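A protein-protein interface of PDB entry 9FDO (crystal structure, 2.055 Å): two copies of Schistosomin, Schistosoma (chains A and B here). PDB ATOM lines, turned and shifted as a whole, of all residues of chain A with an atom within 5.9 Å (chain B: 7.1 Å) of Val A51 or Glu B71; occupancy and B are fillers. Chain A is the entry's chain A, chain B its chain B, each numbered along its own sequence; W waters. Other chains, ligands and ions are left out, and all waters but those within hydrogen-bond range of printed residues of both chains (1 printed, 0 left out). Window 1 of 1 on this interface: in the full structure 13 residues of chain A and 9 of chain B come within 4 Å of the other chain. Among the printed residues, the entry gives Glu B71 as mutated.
The side-chain carboxylate (OE1) of Glu B71 sits at hydrogen-bond distance from the backbone NH (N) of Cys A24 (2.8 Å).
The guanidinium group of Arg B29 is in hydrogen-bond range of the backbone carbonyl oxygen of Val A51, at 3.0 Å.
N of Ser A52 is in hydrogen-bond range of O of Cys A24 (2.9 Å).
The backbone NH (N) of Ser A26 is in hydrogen-bond range of the backbone carbonyl oxygen (O) of Lys A50 (2.9 Å).
OE1 of Glu B43 lies within salt-bridge range of NE of Arg B39, at 2.8 Å.
The guanidinium group (NH1) of Arg B39 sits at hydrogen-bond distance from the backbone carbonyl oxygen (O) of Glu B71, 2.7 Å away.
NH1 of Arg B39 lies within hydrogen-bond range of O of Asp B74, at 2.9 Å.
Arg A22 touches Ser B70.
Phe A23 touches Glu B71 (CA to OE1, 3.2 Å).
Arg B29 touches Lys A50 (NH1 to CE, 3.5 Å).
Glu B71 touches Val A51.
Lys A53 touches Arg B29.
Lys A53 touches Arg B39 (NZ to NH2, 3.97 Å).
Pro A55 touches Glu B71 (CG to OE2, 3.3 Å).
Trp A63 touches Glu B71.
Of chain B, only Arg B29 and Glu B71 come within 4 Å of Val A51.
Of chain A, only Phe A23 (3.2 Å), Cys A24 (2.8 Å), Val A51 (3.4 Å), Pro A55 (3.3 Å) and Trp A63 (3.4 Å) come within 4 Å of Glu B71.
Printed residues of chain A within 4 Å of Arg B29: Lys A50 (3.5 Å), Val A51 (3.0 Å) and Lys A53 (3.6 Å).
Of the printed residues of chain B, Pro A55 touches Glu B71.
Printed residues of chain B within 4 Å of Trp A63: Glu B71 (3.4 Å).
Of the printed residues of chain A, Arg B39 touches Lys A53.
Of the printed residues of chain B, Phe A23 touches Glu B71.
The nearest printed residue of chain B that does not touch Trp A63 is Thr B69 (4.1 Å).
Printed residues of chain B that touch a printed residue of chain A: Arg B29, Arg B39, Ser B70 and Glu B71.
Hydrophobic or aromatic side chains of chain A within 4 Å of the printed part of chain B: Phe A23, Val A51, Pro A55 and Trp A63.
Among the printed residues, no Asp or Glu carboxylate lies within 4 Å of a Lys or Arg side-chain nitrogen of the other chain.
No position is printed for both chains.
Of the 10 pairs that touch across the chains among the printed residues, none has its exchanged pair printed and touching as well.
Water W1 lies within hydrogen-bond range of OG of Ser B70 (2.6 Å), O of Arg A22 (2.7 Å) and N of Glu B71 (2.9 Å).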
ATOM      1  N   ARG A  22     -22.869  -3.324 -30.346  1.00  0.00           N
ATOM      2  CA  ARG A  22     -21.862  -3.360 -29.295  1.00  0.00           C
ATOM      3  C   ARG A  22     -22.262  -2.375 -28.206  1.00  0.00           C
ATOM      4  O   ARG A  22     -22.731  -1.269 -28.498  1.00  0.00           O
ATOM      5  CB  ARG A  22     -20.467  -2.972 -29.829  1.00  0.00           C
ATOM      6  CG  ARG A  22     -19.691  -4.090 -30.463  1.00  0.00           C
ATOM      7  CD  ARG A  22     -20.140  -4.408 -31.882  1.00  0.00           C
ATOM      8  NE  ARG A  22     -19.044  -5.031 -32.619  1.00  0.00           N
ATOM      9  CZ  ARG A  22     -19.163  -5.631 -33.796  1.00  0.00           C
ATOM     10  NH1 ARG A  22     -20.351  -5.707 -34.398  1.00  0.00           N
ATOM     11  NH2 ARG A  22     -18.100  -6.167 -34.381  1.00  0.00           N
ATOM     12  N   PHE A  23     -22.041  -2.757 -26.958  1.00  0.00           N
ATOM     13  CA  PHE A  23     -22.318  -1.879 -25.828  1.00  0.00           C
ATOM     14  C   PHE A  23     -21.242  -1.999 -24.779  1.00  0.00           C
ATOM     15  O   PHE A  23     -21.008  -3.092 -24.279  1.00  0.00           O
ATOM     16  CB  PHE A  23     -23.668  -2.227 -25.148  1.00  0.00           C
ATOM     17  CG  PHE A  23     -24.893  -2.081 -26.023  1.00  0.00           C
ATOM     18  CD1 PHE A  23     -25.504  -0.846 -26.192  1.00  0.00           C
ATOM     19  CD2 PHE A  23     -25.448  -3.179 -26.652  1.00  0.00           C
ATOM     20  CE1 PHE A  23     -26.635  -0.714 -26.994  1.00  0.00           C
ATOM     21  CE2 PHE A  23     -26.584  -3.050 -27.425  1.00  0.00           C
ATOM     22  CZ  PHE A  23     -27.173  -1.821 -27.594  1.00  0.00           C
ATOM     23  N   CYS A  24     -20.659  -0.879 -24.377  1.00  0.00           N
ATOM     24  CA  CYS A  24     -19.768  -0.839 -23.241  1.00  0.00           C
ATOM     25  C   CYS A  24     -20.710  -0.737 -22.037  1.00  0.00           C
ATOM     26  O   CYS A  24     -21.443   0.227 -21.934  1.00  0.00           O
ATOM     27  CB  CYS A  24     -18.841   0.372 -23.301  1.00  0.00           C
ATOM     28  SG  CYS A  24     -17.850   0.593 -21.796  1.00  0.00           S
ATOM     29  N   VAL A  25     -20.761  -1.763 -21.190  1.00  0.00           N
ATOM     30  CA  VAL A  25     -21.614  -1.756 -20.005  1.00  0.00           C
ATOM     31  C   VAL A  25     -20.710  -1.699 -18.768  1.00  0.00           C
ATOM     32  O   VAL A  25     -19.548  -2.127 -18.826  1.00  0.00           O
ATOM     33  CB  VAL A  25     -22.597  -2.961 -19.975  1.00  0.00           C
ATOM     34  CG1 VAL A  25     -23.513  -2.966 -21.218  1.00  0.00           C
ATOM     35  CG2 VAL A  25     -21.858  -4.282 -19.831  1.00  0.00           C
ATOM     36  N   SER A  26     -21.217  -1.164 -17.656  1.00  0.00           N
ATOM     37  CA  SER A  26     -20.428  -1.039 -16.445  1.00  0.00           C
ATOM     38  C   SER A  26     -21.303  -1.361 -15.247  1.00  0.00           C
ATOM     39  O   SER A  26     -22.346  -0.744 -15.079  1.00  0.00           O
ATOM     40  CB  SER A  26     -19.885   0.379 -16.347  1.00  0.00           C
ATOM     41  OG  SER A  26     -19.113   0.539 -15.172  1.00  0.00           O
ATOM     42  N   ARG A  40     -27.100  -7.214 -23.276  1.00  0.00           N
ATOM     43  CA  ARG A  40     -27.152  -5.945 -22.590  1.00  0.00           C
ATOM     44  C   ARG A  40     -28.200  -6.011 -21.484  1.00  0.00           C
ATOM     45  O   ARG A  40     -27.906  -5.594 -20.369  1.00  0.00           O
ATOM     46  CB  ARG A  40     -27.454  -4.815 -23.588  1.00  0.00           C
ATOM     47  CG  ARG A  40     -27.503  -3.448 -22.938  1.00  0.00           C
ATOM     48  CD  ARG A  40     -28.400  -2.564 -23.739  1.00  0.00           C
ATOM     49  NE  ARG A  40     -29.048  -1.542 -22.930  1.00  0.00           N
ATOM     50  CZ  ARG A  40     -29.430  -0.354 -23.396  1.00  0.00           C
ATOM     51  NH1 ARG A  40     -29.220  -0.031 -24.670  1.00  0.00           N
ATOM     52  NH2 ARG A  40     -30.008   0.526 -22.589  1.00  0.00           N
ATOM     53  N   ALA A  49     -25.256  -3.982 -14.521  1.00  0.00           N
ATOM     54  CA  ALA A  49     -24.500  -3.227 -15.498  1.00  0.00           C
ATOM     55  C   ALA A  49     -25.400  -2.352 -16.357  1.00  0.00           C
ATOM     56  O   ALA A  49     -26.372  -2.816 -16.958  1.00  0.00           O
ATOM     57  CB  ALA A  49     -23.672  -4.163 -16.376  1.00  0.00           C
ATOM     58  N   LYS A  50     -25.082  -1.083 -16.389  1.00  0.00           N
ATOM     59  CA  LYS A  50     -25.799  -0.126 -17.205  1.00  0.00           C
ATOM     60  C   LYS A  50     -24.892   0.289 -18.334  1.00  0.00           C
ATOM     61  O   LYS A  50     -23.674   0.256 -18.190  1.00  0.00           O
ATOM     62  CB  LYS A  50     -26.214   1.096 -16.384  1.00  0.00           C
ATOM     63  CG  LYS A  50     -27.061   0.737 -15.180  1.00  0.00           C
ATOM     64  CD  LYS A  50     -26.852   1.703 -13.993  1.00  0.00           C
ATOM     65  CE  LYS A  50     -27.678   2.929 -14.195  1.00  0.00           C
ATOM     66  NZ  LYS A  50     -27.914   3.686 -12.917  1.00  0.00           N
ATOM     67  N   VAL A  51     -25.474   0.728 -19.446  1.00  0.00           N
ATOM     68  CA  VAL A  51     -24.703   1.211 -20.580  1.00  0.00           C
ATOM     69  C   VAL A  51     -23.925   2.457 -20.170  1.00  0.00           C
ATOM     70  O   VAL A  51     -24.490   3.369 -19.562  1.00  0.00           O
ATOM     71  CB  VAL A  51     -25.595   1.467 -21.815  1.00  0.00           C
ATOM     72  CG1 VAL A  51     -24.805   2.147 -22.925  1.00  0.00           C
ATOM     73  CG2 VAL A  51     -26.201   0.171 -22.310  1.00  0.00           C
ATOM     74  N   SER A  52     -22.616   2.429 -20.397  1.00  0.00           N
ATOM     75  CA  SER A  52     -21.713   3.510 -20.033  1.00  0.00           C
ATOM     76  C   SER A  52     -21.969   4.811 -20.777  1.00  0.00           C
ATOM     77  O   SER A  52     -22.160   4.796 -21.986  1.00  0.00           O
ATOM     78  CB  SER A  52     -20.268   3.075 -20.264  1.00  0.00           C
ATOM     79  OG  SER A  52     -19.372   4.090 -19.835  1.00  0.00           O
ATOM     80  N   LYS A  53     -21.928   5.943 -20.064  1.00  0.00           N
ATOM     81  CA  LYS A  53     -22.049   7.252 -20.724  1.00  0.00           C
ATOM     82  C   LYS A  53     -20.681   7.743 -21.259  1.00  0.00           C
ATOM     83  O   LYS A  53     -20.651   8.624 -22.110  1.00  0.00           O
ATOM     84  CB  LYS A  53     -22.728   8.316 -19.850  1.00  0.00           C
ATOM     85  CG  LYS A  53     -24.167   7.982 -19.447  1.00  0.00           C
ATOM     86  CD  LYS A  53     -25.084   7.721 -20.646  1.00  0.00           C
ATOM     87  CE  LYS A  53     -26.250   6.811 -20.331  1.00  0.00           C
ATOM     88  NZ  LYS A  53     -27.073   6.549 -21.546  1.00  0.00           N
ATOM     89  N   PRO A  55     -18.045   5.509 -22.849  1.00  0.00           N
ATOM     90  CA  PRO A  55     -17.480   4.233 -23.326  1.00  0.00           C
ATOM     91  C   PRO A  55     -15.987   4.224 -23.657  1.00  0.00           C
ATOM     92  O   PRO A  55     -15.312   3.228 -23.379  1.00  0.00           O
ATOM     93  CB  PRO A  55     -18.331   3.914 -24.559  1.00  0.00           C
ATOM     94  CG  PRO A  55     -18.953   5.197 -24.948  1.00  0.00           C
ATOM     95  CD  PRO A  55     -19.204   5.899 -23.675  1.00  0.00           C
ATOM     96  N   TRP A  63     -13.954   0.622 -28.576  1.00  0.00           N
ATOM     97  CA  TRP A  63     -14.930  -0.305 -27.993  1.00  0.00           C
ATOM     98  C   TRP A  63     -15.975  -0.750 -29.046  1.00  0.00           C
ATOM     99  O   TRP A  63     -16.553  -1.831 -28.916  1.00  0.00           O
ATOM    100  CB  TRP A  63     -15.647   0.355 -26.778  1.00  0.00           C
ATOM    101  CG  TRP A  63     -16.435   1.575 -27.163  1.00  0.00           C
ATOM    102  CD1 TRP A  63     -15.966   2.848 -27.284  1.00  0.00           C
ATOM    103  CD2 TRP A  63     -17.795   1.599 -27.630  1.00  0.00           C
ATOM    104  NE1 TRP A  63     -16.950   3.673 -27.777  1.00  0.00           N
ATOM    105  CE2 TRP A  63     -18.079   2.925 -28.017  1.00  0.00           C
ATOM    106  CE3 TRP A  63     -18.802   0.629 -27.744  1.00  0.00           C
ATOM    107  CZ2 TRP A  63     -19.326   3.303 -28.519  1.00  0.00           C
ATOM    108  CZ3 TRP A  63     -20.021   0.996 -28.275  1.00  0.00           C
ATOM    109  CH2 TRP A  63     -20.275   2.318 -28.654  1.00  0.00           C
ATOM    110  N   ARG B  29     -27.739  11.695 -15.822  1.00  0.00           N
ATOM    111  CA  ARG B  29     -26.541  10.880 -16.037  1.00  0.00           C
ATOM    112  C   ARG B  29     -25.413  11.644 -16.726  1.00  0.00           C
ATOM    113  O   ARG B  29     -24.484  11.035 -17.242  1.00  0.00           O
ATOM    114  CB  ARG B  29     -26.863   9.605 -16.847  1.00  0.00           C
ATOM    115  CG  ARG B  29     -28.075   8.818 -16.343  1.00  0.00           C
ATOM    116  CD  ARG B  29     -27.815   7.363 -15.918  1.00  0.00           C
ATOM    117  NE  ARG B  29     -26.923   6.630 -16.822  1.00  0.00           N
ATOM    118  CZ  ARG B  29     -25.952   5.812 -16.414  1.00  0.00           C
ATOM    119  NH1 ARG B  29     -25.711   5.648 -15.117  1.00  0.00           N
ATOM    120  NH2 ARG B  29     -25.183   5.191 -17.299  1.00  0.00           N
ATOM    121  N   VAL B  33     -23.375  13.051 -26.230  1.00  0.00           N
ATOM    122  CA  VAL B  33     -23.967  13.173 -27.556  1.00  0.00           C
ATOM    123  C   VAL B  33     -24.777  11.943 -27.918  1.00  0.00           C
ATOM    124  O   VAL B  33     -24.325  10.811 -27.739  1.00  0.00           O
ATOM    125  CB  VAL B  33     -22.911  13.507 -28.629  1.00  0.00           C
ATOM    126  CG1 VAL B  33     -23.525  13.498 -30.032  1.00  0.00           C
ATOM    127  CG2 VAL B  33     -22.247  14.848 -28.327  1.00  0.00           C
ATOM    128  N   ILE B  34     -26.005  12.161 -28.384  1.00  0.00           N
ATOM    129  CA  ILE B  34     -26.832  11.074 -28.889  1.00  0.00           C
ATOM    130  C   ILE B  34     -27.191  11.383 -30.356  1.00  0.00           C
ATOM    131  O   ILE B  34     -26.953  12.500 -30.832  1.00  0.00           O
ATOM    132  CB  ILE B  34     -28.059  10.732 -27.990  1.00  0.00           C
ATOM    133  CG1 ILE B  34     -28.933  11.991 -27.695  1.00  0.00           C
ATOM    134  CG2 ILE B  34     -27.610  10.043 -26.693  1.00  0.00           C
ATOM    135  CD1 ILE B  34     -29.904  12.350 -28.734  1.00  0.00           C
ATOM    136  N   ARG B  39     -34.168   9.120 -29.919  1.00  0.00           N
ATOM    137  CA  ARG B  39     -33.236   8.950 -28.816  1.00  0.00           C
ATOM    138  C   ARG B  39     -33.200  10.171 -27.918  1.00  0.00           C
ATOM    139  O   ARG B  39     -33.075  10.044 -26.710  1.00  0.00           O
ATOM    140  CB  ARG B  39     -31.835   8.543 -29.341  1.00  0.00           C
ATOM    141  CG  ARG B  39     -30.793   8.367 -28.247  1.00  0.00           C
ATOM    142  CD  ARG B  39     -31.160   7.268 -27.263  1.00  0.00           C
ATOM    143  NE  ARG B  39     -30.136   7.165 -26.243  1.00  0.00           N
ATOM    144  CZ  ARG B  39     -29.091   6.351 -26.307  1.00  0.00           C
ATOM    145  NH1 ARG B  39     -28.984   5.473 -27.298  1.00  0.00           N
ATOM    146  NH2 ARG B  39     -28.169   6.373 -25.357  1.00  0.00           N
ATOM    147  N   GLU B  43     -34.125  10.158 -24.010  1.00  0.00           N
ATOM    148  CA  GLU B  43     -33.269  10.765 -22.975  1.00  0.00           C
ATOM    149  C   GLU B  43     -34.029  11.730 -22.075  1.00  0.00           C
ATOM    150  O   GLU B  43     -33.840  11.723 -20.852  1.00  0.00           O
ATOM    151  CB  GLU B  43     -32.059  11.434 -23.622  1.00  0.00           C
ATOM    152  CG  GLU B  43     -31.133  10.421 -24.268  1.00  0.00           C
ATOM    153  CD  GLU B  43     -30.467   9.478 -23.280  1.00  0.00           C
ATOM    154  OE1 GLU B  43     -30.139   8.330 -23.658  1.00  0.00           O
ATOM    155  OE2 GLU B  43     -30.273   9.894 -22.117  1.00  0.00           O
ATOM    156  N   CYS B  68     -22.544   8.168 -35.289  1.00  0.00           N
ATOM    157  CA  CYS B  68     -23.773   7.539 -34.791  1.00  0.00           C
ATOM    158  C   CYS B  68     -23.586   6.027 -34.744  1.00  0.00           C
ATOM    159  O   CYS B  68     -23.330   5.393 -35.764  1.00  0.00           O
ATOM    160  CB  CYS B  68     -24.968   7.907 -35.669  1.00  0.00           C
ATOM    161  SG  CYS B  68     -25.339   9.681 -35.694  1.00  0.00           S
ATOM    162  N   THR B  69     -23.690   5.454 -33.556  1.00  0.00           N
ATOM    163  CA  THR B  69     -23.522   4.011 -33.338  1.00  0.00           C
ATOM    164  C   THR B  69     -24.811   3.456 -32.728  1.00  0.00           C
ATOM    165  O   THR B  69     -25.680   4.241 -32.369  1.00  0.00           O
ATOM    166  CB  THR B  69     -22.340   3.809 -32.352  1.00  0.00           C
ATOM    167  OG1 THR B  69     -22.653   4.535 -31.156  1.00  0.00           O
ATOM    168  CG2 THR B  69     -21.024   4.281 -32.928  1.00  0.00           C
ATOM    169  N   SER B  70     -24.949   2.119 -32.591  1.00  0.00           N
ATOM    170  CA  SER B  70     -26.143   1.553 -31.951  1.00  0.00           C
ATOM    171  C   SER B  70     -26.242   2.044 -30.495  1.00  0.00           C
ATOM    172  O   SER B  70     -27.316   2.453 -30.069  1.00  0.00           O
ATOM    173  CB  SER B  70     -26.141   0.031 -32.029  1.00  0.00           C
ATOM    174  OG  SER B  70     -25.071  -0.489 -31.260  1.00  0.00           O
ATOM    175  N   GLU B  71     -25.106   2.120 -29.785  1.00  0.00           N
ATOM    176  CA  GLU B  71     -25.070   2.633 -28.409  1.00  0.00           C
ATOM    177  C   GLU B  71     -25.659   4.039 -28.210  1.00  0.00           C
ATOM    178  O   GLU B  71     -26.548   4.203 -27.359  1.00  0.00           O
ATOM    179  CB  GLU B  71     -23.659   2.592 -27.827  1.00  0.00           C
ATOM    180  CG  GLU B  71     -23.705   2.655 -26.320  1.00  0.00           C
ATOM    181  CD  GLU B  71     -22.405   2.313 -25.633  1.00  0.00           C
ATOM    182  OE1 GLU B  71     -22.333   1.199 -25.082  1.00  0.00           O
ATOM    183  OE2 GLU B  71     -21.477   3.151 -25.619  1.00  0.00           O
ATOM    184  N   ASN B  72     -25.248   5.025 -29.040  1.00  0.00           N
ATOM    185  CA  ASN B  72     -25.777   6.387 -28.879  1.00  0.00           C
ATOM    186  C   ASN B  72     -27.035   6.674 -29.711  1.00  0.00           C
ATOM    187  O   ASN B  72     -27.593   7.768 -29.611  1.00  0.00           O
ATOM    188  CB  ASN B  72     -24.682   7.470 -29.112  1.00  0.00           C
ATOM    189  CG  ASN B  72     -24.330   7.766 -30.551  1.00  0.00           C
ATOM    190  OD1 ASN B  72     -24.750   7.086 -31.482  1.00  0.00           O
ATOM    191  ND2 ASN B  72     -23.522   8.805 -30.756  1.00  0.00           N
ATOM    192  N   SER B  73     -27.541   5.672 -30.459  1.00  0.00           N
ATOM    193  CA  SER B  73     -28.732   5.868 -31.275  1.00  0.00           C
ATOM    194  C   SER B  73     -29.972   5.127 -30.855  1.00  0.00           C
ATOM    195  O   SER B  73     -31.072   5.656 -31.021  1.00  0.00           O
ATOM    196  CB  SER B  73     -28.432   5.472 -32.704  1.00  0.00           C
ATOM    197  OG  SER B  73     -27.438   6.318 -33.219  1.00  0.00           O
ATOM    198  N   ASP B  74     -29.826   3.863 -30.454  1.00  0.00           N
ATOM    199  CA  ASP B  74     -31.001   3.011 -30.239  1.00  0.00           C
ATOM    200  C   ASP B  74     -31.849   3.401 -29.069  1.00  0.00           C
ATOM    201  O   ASP B  74     -31.333   3.883 -28.059  1.00  0.00           O
ATOM    202  CB  ASP B  74     -30.620   1.528 -30.141  1.00  0.00           C
ATOM    203  CG  ASP B  74     -29.956   0.937 -31.375  1.00  0.00           C
ATOM    204  OD1 ASP B  74     -29.815   1.668 -32.391  1.00  0.00           O
ATOM    205  OD2 ASP B  74     -29.553  -0.240 -31.317  1.00  0.00           O
ATOM    206  N   VAL B  75     -33.169   3.158 -29.209  1.00  0.00           N
ATOM    207  CA  VAL B  75     -34.151   3.368 -28.149  1.00  0.00           C
ATOM    208  C   VAL B  75     -34.833   2.057 -27.831  1.00  0.00           C
ATOM    209  O   VAL B  75     -35.184   1.306 -28.735  1.00  0.00           O
ATOM    210  CB  VAL B  75     -35.161   4.513 -28.418  1.00  0.00           C
ATOM    211  CG1 VAL B  75     -34.430   5.832 -28.520  1.00  0.00           C
ATOM    212  CG2 VAL B  75     -35.975   4.274 -29.680  1.00  0.00           C
HETATM  213  O   HOH W   1     -22.780   0.518 -30.546  1.00  0.00           O
